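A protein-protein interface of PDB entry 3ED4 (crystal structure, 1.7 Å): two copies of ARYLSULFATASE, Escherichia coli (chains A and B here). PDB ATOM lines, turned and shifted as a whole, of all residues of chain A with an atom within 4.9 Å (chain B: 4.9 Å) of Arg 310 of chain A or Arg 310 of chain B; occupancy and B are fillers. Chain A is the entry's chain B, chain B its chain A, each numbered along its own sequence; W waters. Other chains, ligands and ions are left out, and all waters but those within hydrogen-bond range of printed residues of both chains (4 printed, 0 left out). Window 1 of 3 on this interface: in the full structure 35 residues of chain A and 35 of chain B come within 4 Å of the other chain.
OE2 of Glu 311 of chain A lies close to OE2 of Glu 311 of chain B (3.2 Å).
The guanidinium group (NH2) of Arg 310 of chain B is in salt-bridge range of the side-chain carboxylate (OE2) of Glu 323 of chain A (2.9 Å).
The side-chain carboxylate of Glu 323 of chain B lies within salt-bridge range of the guanidinium group of Arg 310 of chain A.
The side-chain carboxylate (OE2) of Glu 323 of chain A is in salt-bridge range of the guanidinium group (NH1) of Arg 310 of chain A (3.7 Å).
N of Glu 311 of chain B sits at hydrogen-bond distance from OG1 of Thr 309 of chain B (3.0 Å).
The guanidinium group (NH1) of Arg 310 of chain B lies within salt-bridge range of the side-chain carboxylate (OE2) of Glu 323 of chain B.
The side-chain hydroxyl (OG1) of Thr 309 of chain A lies within hydrogen-bond range of the backbone NH (N) of Glu 311 of chain A.
Among the printed residues, merely in contact across the chains: Arg 310 of chain A with Arg 310 of chain B (3.5 Å).
Arg 310 of chain A touches just these residues of chain B: Arg 310 and Glu 323.
Arg 310 of chain B touches just these residues of chain A: Arg 310 (3.5 Å) and Glu 323 (2.9 Å).
Of the printed residues of chain B, Glu 311 of chain A touches Glu 311.
Printed residues of chain A within 4 Å of Glu 311 of chain B: Glu 311 (3.2 Å).
Gly 322 of chain B touches none of the printed residues of chain A.
The nearest residue of chain B that does not touch Arg 310 of chain A is Gly 326 of chain B (4.7 Å).
Among the printed residues, 4 pairs touch across the chains.
Among the printed residues, Asp or Glu carboxylates within 4 Å of a Lys or Arg side-chain nitrogen of the other chain: Arg 310 of chain A with Glu 323 of chain B (2.9 Å) and Glu 323 of chain A with Arg 310 of chain B (2.9 Å).
Arg 310 of chain B touches its own counterpart, Arg 310 of chain A.
Arg 310 of chain A touches Glu 323 of chain B, and with the chains exchanged Glu 323 of chain A touches Arg 310 of chain B.
Glu 311 of chain A touches its own counterpart, Glu 311 of chain B.
Positions printed for both chains: 267, 271, 308, 309, 310, 311, 312, 320, 321, 322, 323 and 326.
Of the 4 pairs that touch across the chains among the printed residues, 4 have their exchanged pair printed and touching as well.
Water W1 lies within hydrogen-bond range of O of Gly 326 of chain B and O of Arg 310 of chain A.
Water W2 lies within hydrogen-bond range of O of Gly 326 of chain A (2.9 Å), O of Arg 310 of chain B (3.2 Å) and N of Ala 312 of chain B (3.3 Å).
Water W4 lies within hydrogen-bond range of the side-chain carboxylate (OE2) of Glu 311 of chain A and the side-chain carboxylate (OE2) of Glu 311 of chain B.
Water W3 lies within hydrogen-bond range of the side-chain carboxylate (OE2) of Glu 311 of chain B and the side-chain carboxylate (OE2) of Glu 311 of chain A.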
ATOM      1  N   VAL A 267     -21.085  -5.288  10.965  1.00  0.00           N
ATOM      2  CA  VAL A 267     -20.721  -6.695  11.148  1.00  0.00           C
ATOM      3  C   VAL A 267     -19.541  -7.155  10.268  1.00  0.00           C
ATOM      4  O   VAL A 267     -19.062  -8.290  10.390  1.00  0.00           O
ATOM      5  CB  VAL A 267     -21.971  -7.625  10.995  1.00  0.00           C
ATOM      6  CG1 VAL A 267     -23.059  -7.239  12.004  1.00  0.00           C
ATOM      7  CG2 VAL A 267     -22.526  -7.559   9.597  1.00  0.00           C
ATOM      8  N   TYR A 271     -16.803 -10.655   9.952  1.00  0.00           N
ATOM      9  CA  TYR A 271     -16.761 -11.538   8.769  1.00  0.00           C
ATOM     10  C   TYR A 271     -15.361 -11.605   8.151  1.00  0.00           C
ATOM     11  O   TYR A 271     -14.901 -12.682   7.774  1.00  0.00           O
ATOM     12  CB  TYR A 271     -17.776 -11.108   7.710  1.00  0.00           C
ATOM     13  CG  TYR A 271     -19.221 -11.073   8.155  1.00  0.00           C
ATOM     14  CD1 TYR A 271     -19.658 -11.747   9.310  1.00  0.00           C
ATOM     15  CD2 TYR A 271     -20.157 -10.388   7.400  1.00  0.00           C
ATOM     16  CE1 TYR A 271     -20.970 -11.706   9.701  1.00  0.00           C
ATOM     17  CE2 TYR A 271     -21.472 -10.347   7.776  1.00  0.00           C
ATOM     18  CZ  TYR A 271     -21.880 -10.998   8.932  1.00  0.00           C
ATOM     19  OH  TYR A 271     -23.202 -10.950   9.289  1.00  0.00           O
ATOM     20  N   VAL A 308     -19.189 -14.955  20.474  1.00  0.00           N
ATOM     21  CA  VAL A 308     -19.723 -13.717  20.997  1.00  0.00           C
ATOM     22  C   VAL A 308     -20.584 -13.191  19.857  1.00  0.00           C
ATOM     23  O   VAL A 308     -20.102 -13.008  18.731  1.00  0.00           O
ATOM     24  CB  VAL A 308     -18.616 -12.682  21.333  1.00  0.00           C
ATOM     25  CG1 VAL A 308     -19.248 -11.416  21.827  1.00  0.00           C
ATOM     26  CG2 VAL A 308     -17.643 -13.228  22.354  1.00  0.00           C
ATOM     27  N   THR A 309     -21.867 -12.981  20.141  1.00  0.00           N
ATOM     28  CA  THR A 309     -22.814 -12.567  19.120  1.00  0.00           C
ATOM     29  C   THR A 309     -22.936 -11.051  19.174  1.00  0.00           C
ATOM     30  O   THR A 309     -22.080 -10.378  19.769  1.00  0.00           O
ATOM     31  CB  THR A 309     -24.197 -13.239  19.351  1.00  0.00           C
ATOM     32  OG1 THR A 309     -24.687 -12.843  20.634  1.00  0.00           O
ATOM     33  CG2 THR A 309     -24.080 -14.773  19.333  1.00  0.00           C
ATOM     34  N   ARG A 310     -24.014 -10.515  18.599  1.00  0.00           N
ATOM     35  CA  ARG A 310     -24.393  -9.102  18.805  1.00  0.00           C
ATOM     36  C   ARG A 310     -24.727  -8.798  20.283  1.00  0.00           C
ATOM     37  O   ARG A 310     -24.718  -7.650  20.694  1.00  0.00           O
ATOM     38  CB  ARG A 310     -25.587  -8.727  17.929  1.00  0.00           C
ATOM     39  CG  ARG A 310     -25.300  -8.684  16.421  1.00  0.00           C
ATOM     40  CD  ARG A 310     -26.605  -8.942  15.697  1.00  0.00           C
ATOM     41  NE  ARG A 310     -26.575  -8.599  14.274  1.00  0.00           N
ATOM     42  CZ  ARG A 310     -26.068  -9.384  13.323  1.00  0.00           C
ATOM     43  NH1 ARG A 310     -25.524 -10.559  13.643  1.00  0.00           N
ATOM     44  NH2 ARG A 310     -26.106  -8.998  12.051  1.00  0.00           N
ATOM     45  N   GLU A 311     -25.007  -9.851  21.057  1.00  0.00           N
ATOM     46  CA  GLU A 311     -25.320  -9.772  22.479  1.00  0.00           C
ATOM     47  C   GLU A 311     -24.043  -9.572  23.319  1.00  0.00           C
ATOM     48  O   GLU A 311     -23.551 -10.512  23.955  1.00  0.00           O
ATOM     49  CB  GLU A 311     -26.045 -11.046  22.909  1.00  0.00           C
ATOM     50  CG  GLU A 311     -26.685 -10.960  24.278  1.00  0.00           C
ATOM     51  CD  GLU A 311     -27.353 -12.253  24.688  1.00  0.00           C
ATOM     52  OE1 GLU A 311     -27.501 -13.170  23.844  1.00  0.00           O
ATOM     53  OE2 GLU A 311     -27.760 -12.349  25.878  1.00  0.00           O
ATOM     54  N   ALA A 312     -23.501  -8.355  23.296  1.00  0.00           N
ATOM     55  CA  ALA A 312     -22.279  -8.047  24.033  1.00  0.00           C
ATOM     56  C   ALA A 312     -22.564  -7.903  25.530  1.00  0.00           C
ATOM     57  O   ALA A 312     -23.517  -7.225  25.928  1.00  0.00           O
ATOM     58  CB  ALA A 312     -21.614  -6.800  23.480  1.00  0.00           C
ATOM     59  N   LEU A 320     -19.188  -7.251  17.577  1.00  0.00           N
ATOM     60  CA  LEU A 320     -18.981  -8.603  17.081  1.00  0.00           C
ATOM     61  C   LEU A 320     -20.310  -9.155  16.548  1.00  0.00           C
ATOM     62  O   LEU A 320     -21.353  -8.547  16.756  1.00  0.00           O
ATOM     63  CB  LEU A 320     -18.352  -9.481  18.165  1.00  0.00           C
ATOM     64  CG  LEU A 320     -17.015  -8.972  18.757  1.00  0.00           C
ATOM     65  CD1 LEU A 320     -16.507  -9.835  19.881  1.00  0.00           C
ATOM     66  CD2 LEU A 320     -15.935  -8.810  17.700  1.00  0.00           C
ATOM     67  N   ALA A 321     -20.262 -10.280  15.829  1.00  0.00           N
ATOM     68  CA  ALA A 321     -21.405 -10.685  15.016  1.00  0.00           C
ATOM     69  C   ALA A 321     -21.506 -12.203  14.841  1.00  0.00           C
ATOM     70  O   ALA A 321     -21.960 -12.666  13.796  1.00  0.00           O
ATOM     71  CB  ALA A 321     -21.324  -9.998  13.630  1.00  0.00           C
ATOM     72  N   GLY A 322     -21.090 -12.963  15.864  1.00  0.00           N
ATOM     73  CA  GLY A 322     -21.143 -14.428  15.821  1.00  0.00           C
ATOM     74  C   GLY A 322     -22.532 -14.985  15.580  1.00  0.00           C
ATOM     75  O   GLY A 322     -23.526 -14.376  15.976  1.00  0.00           O
ATOM     76  N   GLU A 323     -22.591 -16.138  14.924  1.00  0.00           N
ATOM     77  CA  GLU A 323     -23.862 -16.757  14.560  1.00  0.00           C
ATOM     78  C   GLU A 323     -23.942 -18.141  15.165  1.00  0.00           C
ATOM     79  O   GLU A 323     -22.940 -18.830  15.244  1.00  0.00           O
ATOM     80  CB  GLU A 323     -23.998 -16.862  13.029  1.00  0.00           C
ATOM     81  CG  GLU A 323     -24.083 -15.524  12.288  1.00  0.00           C
ATOM     82  CD  GLU A 323     -25.461 -14.878  12.318  1.00  0.00           C
ATOM     83  OE1 GLU A 323     -26.433 -15.477  12.835  1.00  0.00           O
ATOM     84  OE2 GLU A 323     -25.561 -13.745  11.814  1.00  0.00           O
ATOM     85  N   GLY A 326     -29.353 -20.004  14.697  1.00  0.00           N
ATOM     86  CA  GLY A 326     -30.600 -19.908  15.455  1.00  0.00           C
ATOM     87  C   GLY A 326     -30.600 -20.556  16.835  1.00  0.00           C
ATOM     88  O   GLY A 326     -31.516 -20.319  17.608  1.00  0.00           O
ATOM     89  N   VAL B 267     -32.363 -15.261   7.824  1.00  0.00           N
ATOM     90  CA  VAL B 267     -32.803 -13.940   8.259  1.00  0.00           C
ATOM     91  C   VAL B 267     -33.693 -13.217   7.218  1.00  0.00           C
ATOM     92  O   VAL B 267     -34.255 -12.158   7.495  1.00  0.00           O
ATOM     93  CB  VAL B 267     -31.590 -13.065   8.698  1.00  0.00           C
ATOM     94  CG1 VAL B 267     -30.820 -13.746   9.841  1.00  0.00           C
ATOM     95  CG2 VAL B 267     -30.666 -12.782   7.535  1.00  0.00           C
ATOM     96  N   TYR B 271     -36.378  -9.663   6.983  1.00  0.00           N
ATOM     97  CA  TYR B 271     -36.098  -8.483   6.163  1.00  0.00           C
ATOM     98  C   TYR B 271     -37.217  -8.218   5.159  1.00  0.00           C
ATOM     99  O   TYR B 271     -37.606  -7.067   4.942  1.00  0.00           O
ATOM    100  CB  TYR B 271     -34.777  -8.596   5.406  1.00  0.00           C
ATOM    101  CG  TYR B 271     -33.530  -8.819   6.226  1.00  0.00           C
ATOM    102  CD1 TYR B 271     -33.471  -8.504   7.593  1.00  0.00           C
ATOM    103  CD2 TYR B 271     -32.378  -9.311   5.610  1.00  0.00           C
ATOM    104  CE1 TYR B 271     -32.302  -8.718   8.331  1.00  0.00           C
ATOM    105  CE2 TYR B 271     -31.203  -9.509   6.331  1.00  0.00           C
ATOM    106  CZ  TYR B 271     -31.174  -9.215   7.686  1.00  0.00           C
ATOM    107  OH  TYR B 271     -30.017  -9.433   8.390  1.00  0.00           O
ATOM    108  N   VAL B 308     -37.456  -8.454  18.552  1.00  0.00           N
ATOM    109  CA  VAL B 308     -37.037  -9.816  18.782  1.00  0.00           C
ATOM    110  C   VAL B 308     -35.857 -10.020  17.835  1.00  0.00           C
ATOM    111  O   VAL B 308     -35.979  -9.868  16.609  1.00  0.00           O
ATOM    112  CB  VAL B 308     -38.142 -10.850  18.481  1.00  0.00           C
ATOM    113  CG1 VAL B 308     -37.634 -12.238  18.818  1.00  0.00           C
ATOM    114  CG2 VAL B 308     -39.384 -10.543  19.276  1.00  0.00           C
ATOM    115  N   THR B 309     -34.709 -10.348  18.416  1.00  0.00           N
ATOM    116  CA  THR B 309     -33.486 -10.545  17.661  1.00  0.00           C
ATOM    117  C   THR B 309     -33.277 -12.028  17.387  1.00  0.00           C
ATOM    118  O   THR B 309     -34.227 -12.811  17.466  1.00  0.00           O
ATOM    119  CB  THR B 309     -32.314 -10.009  18.493  1.00  0.00           C
ATOM    120  OG1 THR B 309     -32.205 -10.809  19.680  1.00  0.00           O
ATOM    121  CG2 THR B 309     -32.572  -8.552  18.870  1.00  0.00           C
ATOM    122  N   ARG B 310     -32.032 -12.420  17.094  1.00  0.00           N
ATOM    123  CA  ARG B 310     -31.660 -13.838  16.995  1.00  0.00           C
ATOM    124  C   ARG B 310     -31.758 -14.539  18.359  1.00  0.00           C
ATOM    125  O   ARG B 310     -31.718 -15.764  18.434  1.00  0.00           O
ATOM    126  CB  ARG B 310     -30.245 -14.000  16.448  1.00  0.00           C
ATOM    127  CG  ARG B 310     -30.079 -13.639  14.997  1.00  0.00           C
ATOM    128  CD  ARG B 310     -28.644 -13.200  14.787  1.00  0.00           C
ATOM    129  NE  ARG B 310     -28.244 -13.213  13.385  1.00  0.00           N
ATOM    130  CZ  ARG B 310     -28.432 -12.213  12.533  1.00  0.00           C
ATOM    131  NH1 ARG B 310     -29.037 -11.098  12.922  1.00  0.00           N
ATOM    132  NH2 ARG B 310     -27.995 -12.326  11.288  1.00  0.00           N
ATOM    133  N   GLU B 311     -31.877 -13.741  19.420  1.00  0.00           N
ATOM    134  CA  GLU B 311     -32.003 -14.229  20.792  1.00  0.00           C
ATOM    135  C   GLU B 311     -33.472 -14.571  21.112  1.00  0.00           C
ATOM    136  O   GLU B 311     -34.155 -13.812  21.807  1.00  0.00           O
ATOM    137  CB  GLU B 311     -31.455 -13.160  21.752  1.00  0.00           C
ATOM    138  CG  GLU B 311     -31.238 -13.602  23.191  1.00  0.00           C
ATOM    139  CD  GLU B 311     -30.831 -12.451  24.112  1.00  0.00           C
ATOM    140  OE1 GLU B 311     -30.444 -11.360  23.643  1.00  0.00           O
ATOM    141  OE2 GLU B 311     -30.877 -12.650  25.343  1.00  0.00           O
ATOM    142  N   ALA B 312     -33.949 -15.700  20.578  1.00  0.00           N
ATOM    143  CA  ALA B 312     -35.315 -16.177  20.838  1.00  0.00           C
ATOM    144  C   ALA B 312     -35.446 -16.764  22.241  1.00  0.00           C
ATOM    145  O   ALA B 312     -34.611 -17.567  22.675  1.00  0.00           O
ATOM    146  CB  ALA B 312     -35.763 -17.189  19.787  1.00  0.00           C
ATOM    147  N   LEU B 320     -36.308 -15.003  13.670  1.00  0.00           N
ATOM    148  CA  LEU B 320     -36.418 -13.555  13.522  1.00  0.00           C
ATOM    149  C   LEU B 320     -34.999 -12.964  13.625  1.00  0.00           C
ATOM    150  O   LEU B 320     -34.066 -13.679  13.985  1.00  0.00           O
ATOM    151  CB  LEU B 320     -37.370 -12.981  14.581  1.00  0.00           C
ATOM    152  CG  LEU B 320     -38.743 -13.689  14.673  1.00  0.00           C
ATOM    153  CD1 LEU B 320     -39.594 -13.199  15.812  1.00  0.00           C
ATOM    154  CD2 LEU B 320     -39.506 -13.554  13.373  1.00  0.00           C
ATOM    155  N   ALA B 321     -34.833 -11.687  13.284  1.00  0.00           N
ATOM    156  CA  ALA B 321     -33.491 -11.126  13.096  1.00  0.00           C
ATOM    157  C   ALA B 321     -33.430  -9.610  13.334  1.00  0.00           C
ATOM    158  O   ALA B 321     -32.748  -8.886  12.595  1.00  0.00           O
ATOM    159  CB  ALA B 321     -32.973 -11.470  11.698  1.00  0.00           C
ATOM    160  N   GLY B 322     -34.157  -9.141  14.343  1.00  0.00           N
ATOM    161  CA  GLY B 322     -34.138  -7.734  14.741  1.00  0.00           C
ATOM    162  C   GLY B 322     -32.753  -7.231  15.073  1.00  0.00           C
ATOM    163  O   GLY B 322     -31.893  -7.985  15.529  1.00  0.00           O
ATOM    164  N   GLU B 323     -32.546  -5.949  14.820  1.00  0.00           N
ATOM    165  CA  GLU B 323     -31.255  -5.329  15.040  1.00  0.00           C
ATOM    166  C   GLU B 323     -31.411  -4.142  16.003  1.00  0.00           C
ATOM    167  O   GLU B 323     -32.414  -3.430  15.977  1.00  0.00           O
ATOM    168  CB  GLU B 323     -30.673  -4.842  13.695  1.00  0.00           C
ATOM    169  CG  GLU B 323     -30.292  -5.951  12.690  1.00  0.00           C
ATOM    170  CD  GLU B 323     -28.938  -6.600  12.957  1.00  0.00           C
ATOM    171  OE1 GLU B 323     -28.271  -6.249  13.947  1.00  0.00           O
ATOM    172  OE2 GLU B 323     -28.538  -7.481  12.155  1.00  0.00           O
ATOM    173  N   GLY B 326     -26.194  -2.366  17.666  1.00  0.00           N
ATOM    174  CA  GLY B 326     -25.245  -2.701  18.719  1.00  0.00           C
ATOM    175  C   GLY B 326     -25.738  -2.504  20.144  1.00  0.00           C
ATOM    176  O   GLY B 326     -25.101  -2.993  21.062  1.00  0.00           O
HETATM  177  O   HOH W   1     -24.955  -5.158  22.771  1.00  0.00           O
HETATM  178  O   HOH W   2     -32.413 -18.538  19.766  1.00  0.00           O
HETATM  179  O   HOH W   3     -29.380 -14.852  27.073  1.00  0.00           O
HETATM  180  O   HOH W   4     -29.756 -10.798  27.685  1.00  0.00           O
